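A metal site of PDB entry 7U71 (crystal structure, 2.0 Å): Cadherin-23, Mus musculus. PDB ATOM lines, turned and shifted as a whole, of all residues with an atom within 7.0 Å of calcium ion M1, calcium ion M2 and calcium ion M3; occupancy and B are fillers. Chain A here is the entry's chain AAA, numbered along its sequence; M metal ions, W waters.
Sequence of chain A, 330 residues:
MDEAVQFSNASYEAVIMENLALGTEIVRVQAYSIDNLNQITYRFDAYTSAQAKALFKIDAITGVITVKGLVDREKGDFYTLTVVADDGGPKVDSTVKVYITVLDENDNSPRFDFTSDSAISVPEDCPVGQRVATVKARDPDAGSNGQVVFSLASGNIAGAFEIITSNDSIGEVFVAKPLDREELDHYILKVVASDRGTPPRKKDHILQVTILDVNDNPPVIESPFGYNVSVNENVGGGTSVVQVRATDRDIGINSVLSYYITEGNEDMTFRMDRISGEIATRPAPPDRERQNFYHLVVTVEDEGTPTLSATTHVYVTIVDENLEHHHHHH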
ATOM      1  N   GLU A  18      11.177   8.389  -6.852  1.00  0.00           N
ATOM      2  CA  GLU A  18      11.698   7.479  -7.896  1.00  0.00           C
ATOM      3  C   GLU A  18      10.764   6.254  -8.010  1.00  0.00           C
ATOM      4  O   GLU A  18      10.032   5.969  -7.041  1.00  0.00           O
ATOM      5  CB  GLU A  18      13.147   7.085  -7.629  1.00  0.00           C
ATOM      6  CG  GLU A  18      13.368   6.261  -6.368  1.00  0.00           C
ATOM      7  CD  GLU A  18      14.788   5.758  -6.313  1.00  0.00           C
ATOM      8  OE1 GLU A  18      15.340   5.621  -5.180  1.00  0.00           O
ATOM      9  OE2 GLU A  18      15.358   5.500  -7.437  1.00  0.00           O
ATOM     10  N   ASN A  19      10.766   5.613  -9.183  1.00  0.00           N
ATOM     11  CA  ASN A  19      10.042   4.347  -9.464  1.00  0.00           C
ATOM     12  C   ASN A  19       8.524   4.627  -9.511  1.00  0.00           C
ATOM     13  O   ASN A  19       7.739   3.685  -9.460  1.00  0.00           O
ATOM     14  CB  ASN A  19      10.379   3.262  -8.448  1.00  0.00           C
ATOM     15  CG  ASN A  19      11.872   3.009  -8.374  1.00  0.00           C
ATOM     16  OD1 ASN A  19      12.553   2.975  -9.397  1.00  0.00           O
ATOM     17  ND2 ASN A  19      12.403   2.913  -7.175  1.00  0.00           N
ATOM     18  N   VAL A  71      11.920   6.347 -13.679  1.00  0.00           N
ATOM     19  CA  VAL A  71      12.631   7.433 -12.944  1.00  0.00           C
ATOM     20  C   VAL A  71      13.432   6.777 -11.794  1.00  0.00           C
ATOM     21  O   VAL A  71      12.834   6.170 -10.893  1.00  0.00           O
ATOM     22  CB  VAL A  71      11.637   8.499 -12.442  1.00  0.00           C
ATOM     23  CG1 VAL A  71      12.342   9.621 -11.707  1.00  0.00           C
ATOM     24  CG2 VAL A  71      10.791   9.047 -13.602  1.00  0.00           C
ATOM     25  N   ASP A  72      14.747   6.840 -11.907  1.00  0.00           N
ATOM     26  CA  ASP A  72      15.730   6.171 -11.020  1.00  0.00           C
ATOM     27  C   ASP A  72      16.597   7.289 -10.425  1.00  0.00           C
ATOM     28  O   ASP A  72      17.448   7.822 -11.151  1.00  0.00           O
ATOM     29  CB  ASP A  72      16.644   5.219 -11.791  1.00  0.00           C
ATOM     30  CG  ASP A  72      17.616   4.426 -10.908  1.00  0.00           C
ATOM     31  OD1 ASP A  72      17.706   4.691  -9.680  1.00  0.00           O
ATOM     32  OD2 ASP A  72      18.299   3.571 -11.479  1.00  0.00           O
ATOM     33  N   ARG A  73      16.425   7.596  -9.147  1.00  0.00           N
ATOM     34  CA  ARG A  73      17.224   8.669  -8.498  1.00  0.00           C
ATOM     35  C   ARG A  73      18.711   8.336  -8.615  1.00  0.00           C
ATOM     36  O   ARG A  73      19.471   9.289  -8.629  1.00  0.00           O
ATOM     37  CB  ARG A  73      16.880   8.819  -7.013  1.00  0.00           C
ATOM     38  CG  ARG A  73      17.418  10.078  -6.372  1.00  0.00           C
ATOM     39  CD  ARG A  73      17.599   9.958  -4.866  1.00  0.00           C
ATOM     40  NE  ARG A  73      18.657   9.006  -4.613  1.00  0.00           N
ATOM     41  CZ  ARG A  73      19.964   9.227  -4.650  1.00  0.00           C
ATOM     42  NH1 ARG A  73      20.447  10.446  -4.763  1.00  0.00           N
ATOM     43  NH2 ARG A  73      20.783   8.208  -4.477  1.00  0.00           N
ATOM     44  N   GLU A  74      19.092   7.053  -8.570  1.00  0.00           N
ATOM     45  CA  GLU A  74      20.528   6.693  -8.629  1.00  0.00           C
ATOM     46  C   GLU A  74      21.069   7.024 -10.022  1.00  0.00           C
ATOM     47  O   GLU A  74      22.312   6.969 -10.155  1.00  0.00           O
ATOM     48  CB  GLU A  74      20.763   5.222  -8.246  1.00  0.00           C
ATOM     49  CG  GLU A  74      20.648   4.983  -6.746  1.00  0.00           C
ATOM     50  CD  GLU A  74      19.262   5.101  -6.136  1.00  0.00           C
ATOM     51  OE1 GLU A  74      18.324   4.386  -6.570  1.00  0.00           O
ATOM     52  OE2 GLU A  74      19.128   5.912  -5.192  1.00  0.00           O
ATOM     53  N   LYS A  75      20.217   7.342 -11.020  1.00  0.00           N
ATOM     54  CA  LYS A  75      20.714   7.802 -12.360  1.00  0.00           C
ATOM     55  C   LYS A  75      20.599   9.318 -12.513  1.00  0.00           C
ATOM     56  O   LYS A  75      21.105   9.825 -13.495  1.00  0.00           O
ATOM     57  CB  LYS A  75      19.953   7.095 -13.494  1.00  0.00           C
ATOM     58  CG  LYS A  75      20.337   5.643 -13.701  1.00  0.00           C
ATOM     59  CD  LYS A  75      19.608   5.017 -14.883  1.00  0.00           C
ATOM     60  CE  LYS A  75      19.364   3.531 -14.737  1.00  0.00           C
ATOM     61  NZ  LYS A  75      20.627   2.766 -14.633  1.00  0.00           N
ATOM     62  N   LEU A 103      12.921  12.166  -5.474  1.00  0.00           N
ATOM     63  CA  LEU A 103      13.275  11.693  -4.106  1.00  0.00           C
ATOM     64  C   LEU A 103      13.672  10.207  -4.132  1.00  0.00           C
ATOM     65  O   LEU A 103      13.348   9.473  -5.069  1.00  0.00           O
ATOM     66  CB  LEU A 103      12.096  11.966  -3.153  1.00  0.00           C
ATOM     67  CG  LEU A 103      11.587  13.399  -3.135  1.00  0.00           C
ATOM     68  CD1 LEU A 103      10.403  13.492  -2.162  1.00  0.00           C
ATOM     69  CD2 LEU A 103      12.705  14.335  -2.706  1.00  0.00           C
ATOM     70  N   ASP A 104      14.342   9.790  -3.074  1.00  0.00           N
ATOM     71  CA  ASP A 104      14.965   8.461  -2.900  1.00  0.00           C
ATOM     72  C   ASP A 104      13.973   7.455  -2.335  1.00  0.00           C
ATOM     73  O   ASP A 104      13.345   7.752  -1.343  1.00  0.00           O
ATOM     74  CB  ASP A 104      16.133   8.553  -1.936  1.00  0.00           C
ATOM     75  CG  ASP A 104      16.989   7.304  -1.932  1.00  0.00           C
ATOM     76  OD1 ASP A 104      17.262   6.777  -3.014  1.00  0.00           O
ATOM     77  OD2 ASP A 104      17.392   6.894  -0.839  1.00  0.00           O
ATOM     78  N   GLU A 105      13.893   6.290  -2.926  1.00  0.00           N
ATOM     79  CA  GLU A 105      13.390   5.038  -2.300  1.00  0.00           C
ATOM     80  C   GLU A 105      14.586   4.208  -1.814  1.00  0.00           C
ATOM     81  O   GLU A 105      15.658   4.241  -2.455  1.00  0.00           O
ATOM     82  CB  GLU A 105      12.612   4.186  -3.306  1.00  0.00           C
ATOM     83  CG  GLU A 105      11.300   4.816  -3.729  1.00  0.00           C
ATOM     84  CD  GLU A 105      10.267   3.825  -4.253  1.00  0.00           C
ATOM     85  OE1 GLU A 105      10.651   2.858  -4.945  1.00  0.00           O
ATOM     86  OE2 GLU A 105       9.059   4.052  -3.961  1.00  0.00           O
ATOM     87  N   ASN A 106      14.424   3.514  -0.714  1.00  0.00           N
ATOM     88  CA  ASN A 106      15.415   2.514  -0.271  1.00  0.00           C
ATOM     89  C   ASN A 106      15.293   1.305  -1.190  1.00  0.00           C
ATOM     90  O   ASN A 106      14.804   0.245  -0.748  1.00  0.00           O
ATOM     91  CB  ASN A 106      15.254   2.129   1.183  1.00  0.00           C
ATOM     92  CG  ASN A 106      16.505   1.414   1.651  1.00  0.00           C
ATOM     93  OD1 ASN A 106      17.568   1.505   1.007  1.00  0.00           O
ATOM     94  ND2 ASN A 106      16.381   0.673   2.729  1.00  0.00           N
ATOM     95  N   ASP A 107      15.744   1.427  -2.449  1.00  0.00           N
ATOM     96  CA  ASP A 107      15.557   0.346  -3.438  1.00  0.00           C
ATOM     97  C   ASP A 107      16.868  -0.383  -3.686  1.00  0.00           C
ATOM     98  O   ASP A 107      16.875  -1.250  -4.566  1.00  0.00           O
ATOM     99  CB  ASP A 107      14.877   0.857  -4.715  1.00  0.00           C
ATOM    100  CG  ASP A 107      15.591   1.981  -5.476  1.00  0.00           C
ATOM    101  OD1 ASP A 107      16.516   2.653  -4.906  1.00  0.00           O
ATOM    102  OD2 ASP A 107      15.166   2.217  -6.627  1.00  0.00           O
ATOM    103  N   ASN A 108      17.925  -0.143  -2.897  1.00  0.00           N
ATOM    104  CA  ASN A 108      19.201  -0.869  -3.081  1.00  0.00           C
ATOM    105  C   ASN A 108      19.642  -1.441  -1.731  1.00  0.00           C
ATOM    106  O   ASN A 108      19.377  -0.818  -0.687  1.00  0.00           O
ATOM    107  CB  ASN A 108      20.286   0.010  -3.705  1.00  0.00           C
ATOM    108  CG  ASN A 108      19.961   0.392  -5.141  1.00  0.00           C
ATOM    109  OD1 ASN A 108      20.298  -0.369  -6.059  1.00  0.00           O
ATOM    110  ND2 ASN A 108      19.216   1.466  -5.350  1.00  0.00           N
ATOM    111  N   SER A 109      20.211  -2.654  -1.774  1.00  0.00           N
ATOM    112  CA  SER A 109      20.822  -3.327  -0.619  1.00  0.00           C
ATOM    113  C   SER A 109      22.312  -3.029  -0.677  1.00  0.00           C
ATOM    114  O   SER A 109      22.812  -2.711  -1.742  1.00  0.00           O
ATOM    115  CB  SER A 109      20.582  -4.844  -0.609  1.00  0.00           C
ATOM    116  OG  SER A 109      19.202  -5.073  -0.663  1.00  0.00           O
ATOM    117  N   PRO A 110      23.025  -3.092   0.470  1.00  0.00           N
ATOM    118  CA  PRO A 110      24.478  -3.037   0.432  1.00  0.00           C
ATOM    119  C   PRO A 110      25.031  -4.198  -0.395  1.00  0.00           C
ATOM    120  O   PRO A 110      24.453  -5.269  -0.406  1.00  0.00           O
ATOM    121  CB  PRO A 110      24.853  -3.153   1.896  1.00  0.00           C
ATOM    122  CG  PRO A 110      23.633  -2.665   2.690  1.00  0.00           C
ATOM    123  CD  PRO A 110      22.457  -3.094   1.836  1.00  0.00           C
ATOM    124  N   ASP A 139      26.268   1.110  -0.762  1.00  0.00           N
ATOM    125  CA  ASP A 139      24.805   1.211  -0.924  1.00  0.00           C
ATOM    126  C   ASP A 139      24.597   2.562  -1.599  1.00  0.00           C
ATOM    127  O   ASP A 139      25.030   3.575  -1.092  1.00  0.00           O
ATOM    128  CB  ASP A 139      24.093   1.092   0.435  1.00  0.00           C
ATOM    129  CG  ASP A 139      22.582   1.029   0.288  1.00  0.00           C
ATOM    130  OD1 ASP A 139      22.038   1.835  -0.497  1.00  0.00           O
ATOM    131  OD2 ASP A 139      21.958   0.154   0.973  1.00  0.00           O
ATOM    132  N   PRO A 140      24.108   2.591  -2.831  1.00  0.00           N
ATOM    133  CA  PRO A 140      24.051   3.849  -3.577  1.00  0.00           C
ATOM    134  C   PRO A 140      22.792   4.682  -3.292  1.00  0.00           C
ATOM    135  O   PRO A 140      22.628   5.722  -3.913  1.00  0.00           O
ATOM    136  CB  PRO A 140      24.074   3.324  -5.015  1.00  0.00           C
ATOM    137  CG  PRO A 140      23.299   2.038  -4.954  1.00  0.00           C
ATOM    138  CD  PRO A 140      23.656   1.426  -3.616  1.00  0.00           C
ATOM    139  N   ASP A 141      21.947   4.279  -2.336  1.00  0.00           N
ATOM    140  CA  ASP A 141      20.791   5.133  -1.963  1.00  0.00           C
ATOM    141  C   ASP A 141      21.292   6.406  -1.240  1.00  0.00           C
ATOM    142  O   ASP A 141      22.491   6.502  -0.888  1.00  0.00           O
ATOM    143  CB  ASP A 141      19.753   4.339  -1.182  1.00  0.00           C
ATOM    144  CG  ASP A 141      19.155   3.200  -1.959  1.00  0.00           C
ATOM    145  OD1 ASP A 141      18.848   3.411  -3.148  1.00  0.00           O
ATOM    146  OD2 ASP A 141      19.053   2.069  -1.395  1.00  0.00           O
ATOM    147  N   ALA A 142      20.403   7.328  -0.916  1.00  0.00           N
ATOM    148  CA  ALA A 142      20.733   8.651  -0.327  1.00  0.00           C
ATOM    149  C   ALA A 142      20.542   8.571   1.189  1.00  0.00           C
ATOM    150  O   ALA A 142      19.688   7.768   1.657  1.00  0.00           O
ATOM    151  CB  ALA A 142      19.872   9.750  -0.968  1.00  0.00           C
ATOM    152  N   SER A 144      20.359   8.001   5.038  1.00  0.00           N
ATOM    153  CA  SER A 144      20.244   6.771   5.871  1.00  0.00           C
ATOM    154  C   SER A 144      20.138   5.506   4.991  1.00  0.00           C
ATOM    155  O   SER A 144      20.677   4.448   5.348  1.00  0.00           O
ATOM    156  CB  SER A 144      18.998   6.855   6.732  1.00  0.00           C
ATOM    157  OG  SER A 144      19.154   7.788   7.776  1.00  0.00           O
ATOM    158  N   ASN A 145      19.325   5.585   3.938  1.00  0.00           N
ATOM    159  CA  ASN A 145      19.070   4.474   2.969  1.00  0.00           C
ATOM    160  C   ASN A 145      20.379   3.982   2.373  1.00  0.00           C
ATOM    161  O   ASN A 145      20.399   2.838   1.905  1.00  0.00           O
ATOM    162  CB  ASN A 145      18.135   4.866   1.824  1.00  0.00           C
ATOM    163  CG  ASN A 145      16.750   5.237   2.306  1.00  0.00           C
ATOM    164  OD1 ASN A 145      16.317   4.804   3.386  1.00  0.00           O
ATOM    165  ND2 ASN A 145      16.037   6.027   1.505  1.00  0.00           N
ATOM    166  N   GLY A 146      21.418   4.822   2.381  1.00  0.00           N
ATOM    167  CA  GLY A 146      22.733   4.485   1.817  1.00  0.00           C
ATOM    168  C   GLY A 146      23.843   4.330   2.837  1.00  0.00           C
ATOM    169  O   GLY A 146      24.971   4.022   2.416  1.00  0.00           O
ATOM    170  N   GLN A 147      23.597   4.589   4.110  1.00  0.00           N
ATOM    171  CA  GLN A 147      24.650   4.400   5.142  1.00  0.00           C
ATOM    172  C   GLN A 147      24.766   2.920   5.512  1.00  0.00           C
ATOM    173  O   GLN A 147      23.723   2.338   5.744  1.00  0.00           O
ATOM    174  CB  GLN A 147      24.234   5.119   6.424  1.00  0.00           C
ATOM    175  CG  GLN A 147      24.421   6.611   6.350  1.00  0.00           C
ATOM    176  CD  GLN A 147      23.889   7.225   7.621  1.00  0.00           C
ATOM    177  OE1 GLN A 147      22.913   6.780   8.209  1.00  0.00           O
ATOM    178  NE2 GLN A 147      24.598   8.229   8.107  1.00  0.00           N
ATOM    179  N   ASP A 195      21.934  -1.452   5.669  1.00  0.00           N
ATOM    180  CA  ASP A 195      21.754   0.016   5.525  1.00  0.00           C
ATOM    181  C   ASP A 195      20.987   0.536   6.747  1.00  0.00           C
ATOM    182  O   ASP A 195      20.696  -0.238   7.674  1.00  0.00           O
ATOM    183  CB  ASP A 195      21.177   0.422   4.165  1.00  0.00           C
ATOM    184  CG  ASP A 195      19.734   0.032   3.880  1.00  0.00           C
ATOM    185  OD1 ASP A 195      18.933  -0.137   4.871  1.00  0.00           O
ATOM    186  OD2 ASP A 195      19.422  -0.109   2.655  1.00  0.00           O
ATOM    187  N   ARG A 196      20.708   1.833   6.795  1.00  0.00           N
ATOM    188  CA  ARG A 196      19.937   2.425   7.909  1.00  0.00           C
ATOM    189  C   ARG A 196      18.581   2.861   7.365  1.00  0.00           C
ATOM    190  O   ARG A 196      17.989   3.797   7.898  1.00  0.00           O
ATOM    191  CB  ARG A 196      20.761   3.542   8.545  1.00  0.00           C
ATOM    192  CG  ARG A 196      22.004   3.036   9.273  1.00  0.00           C
ATOM    193  CD  ARG A 196      22.458   3.966  10.392  1.00  0.00           C
ATOM    194  NE  ARG A 196      23.812   3.698  10.898  1.00  0.00           N
ATOM    195  CZ  ARG A 196      24.138   2.949  11.947  1.00  0.00           C
ATOM    196  NH1 ARG A 196      23.220   2.336  12.654  1.00  0.00           N
ATOM    197  NH2 ARG A 196      25.416   2.843  12.311  1.00  0.00           N
ATOM    198  N   GLY A 197      18.104   2.169   6.352  1.00  0.00           N
ATOM    199  CA  GLY A 197      16.725   2.366   5.924  1.00  0.00           C
ATOM    200  C   GLY A 197      15.785   1.980   7.045  1.00  0.00           C
ATOM    201  O   GLY A 197      16.182   1.227   7.952  1.00  0.00           O
ATOM    202  N   ARG A 201      17.683  -2.697   4.745  1.00  0.00           N
ATOM    203  CA  ARG A 201      18.029  -3.771   3.791  1.00  0.00           C
ATOM    204  C   ARG A 201      19.397  -4.337   4.156  1.00  0.00           C
ATOM    205  O   ARG A 201      20.303  -3.573   4.506  1.00  0.00           O
ATOM    206  CB  ARG A 201      17.930  -3.165   2.402  1.00  0.00           C
ATOM    207  CG  ARG A 201      16.489  -2.943   1.948  1.00  0.00           C
ATOM    208  CD  ARG A 201      16.466  -2.261   0.607  1.00  0.00           C
ATOM    209  NE  ARG A 201      16.817  -3.194  -0.426  1.00  0.00           N
ATOM    210  CZ  ARG A 201      16.126  -3.428  -1.532  1.00  0.00           C
ATOM    211  NH1 ARG A 201      15.014  -2.776  -1.827  1.00  0.00           N
ATOM    212  NH2 ARG A 201      16.562  -4.353  -2.351  1.00  0.00           N
HETATM  213 CA    CA M   1      16.634   3.599  -7.878  1.00  0.00          CA
HETATM  214 CA    CA M   2      17.211   4.802  -4.205  1.00  0.00          CA
HETATM  215 CA    CA M   3      19.895   1.028   0.617  1.00  0.00          CA
HETATM  216  O   HOH W   1      15.232   2.930  -9.649  1.00  0.00           O
HETATM  217  O   HOH W   2      18.269   1.711  -8.245  1.00  0.00           O
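The side-chain carboxylate (OE2) of Glu 18 lies close to the backbone NH (N) of Arg 73 (2.9 Å). The side-chain carboxylate of Glu 74 sits close to the side-chain amide nitrogen of Asn 108, 3.3 Å away. OD1 of Asp 104 sits close to NE of Arg 73 (3.1 Å). The side-chain amide nitrogen of Asn 108 lies close to the side-chain carboxylate of Asp 107, at 3.0 Å. The side-chain amide nitrogen (ND2) of Asn 19 lies close to the side-chain carboxylate (OD2) of Asp 107. OD1 of Asp 195 is in hydrogen-bond range of N of Gly 197. The side-chain carboxylate (OE1) of Glu 105 is in hydrogen-bond range of the side-chain amide nitrogen (ND2) of Asn 19 (2.8 Å). The backbone carbonyl oxygen of Asn 106 lies within hydrogen-bond range of the guanidinium group of Arg 201 (3.2 Å).
Four residues have an atom within 4 Å of calcium ion M1: Glu 18, Asp 72, Glu 74 and Asp 107.
Six residues have an atom within 4 Å of calcium ion M2: Glu 18, Glu 74, Asp 104, Glu 105, Asp 107 and Asp 141. The nearest printed residue that does not touch calcium ion M2 is Asn 108 (4.1 Å).
OE1 of Glu 74 binds calcium ion M1 (2.3 Å). The side-chain carboxylate (OE2) of Glu 18 binds calcium ion M1 (2.3 Å). Water W1 is bound to calcium ion M1, 2.4 Å away. The side-chain carboxylate (OD1) of Asp 72 binds calcium ion M1 (2.4 Å). Calcium ion M1 is bound by OD2 of Asp 107 (2.4 Å). Calcium ion M1 is bound by water W2. Calcium ion M1 has six donor atoms within binding distance. Slightly farther from calcium ion M1 lies OD1 of Asp 107 (3.1 Å).
Calcium ion M2 is bound by the side-chain carboxylate (OE1) of Glu 18, the side-chain carboxylate (OD1) of Asp 104, the side-chain carboxylate (OD1) of Asp 107, the side-chain carboxylate (OD1) of Asp 141, the backbone carbonyl oxygen (O) of Glu 105, the side-chain carboxylate (OE2) of Glu 74 and the side-chain carboxylate (OE1) of Glu 74.
Calcium ion M3 is bound by the side-chain carboxylate (OD2) of Asp 139 (2.3 Å), the backbone carbonyl oxygen (O) of Asn 145 (2.3 Å), the backbone carbonyl oxygen (O) of Asn 108 (2.3 Å), the side-chain carboxylate (OD2) of Asp 195 (2.4 Å), the side-chain amide oxygen (OD1) of Asn 106 (2.4 Å), the side-chain carboxylate (OD2) of Asp 141 (2.4 Å) and the side-chain carboxylate (OD1) of Asp 139 (2.5 Å). Calcium ion M3 has seven donor atoms within binding distance.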
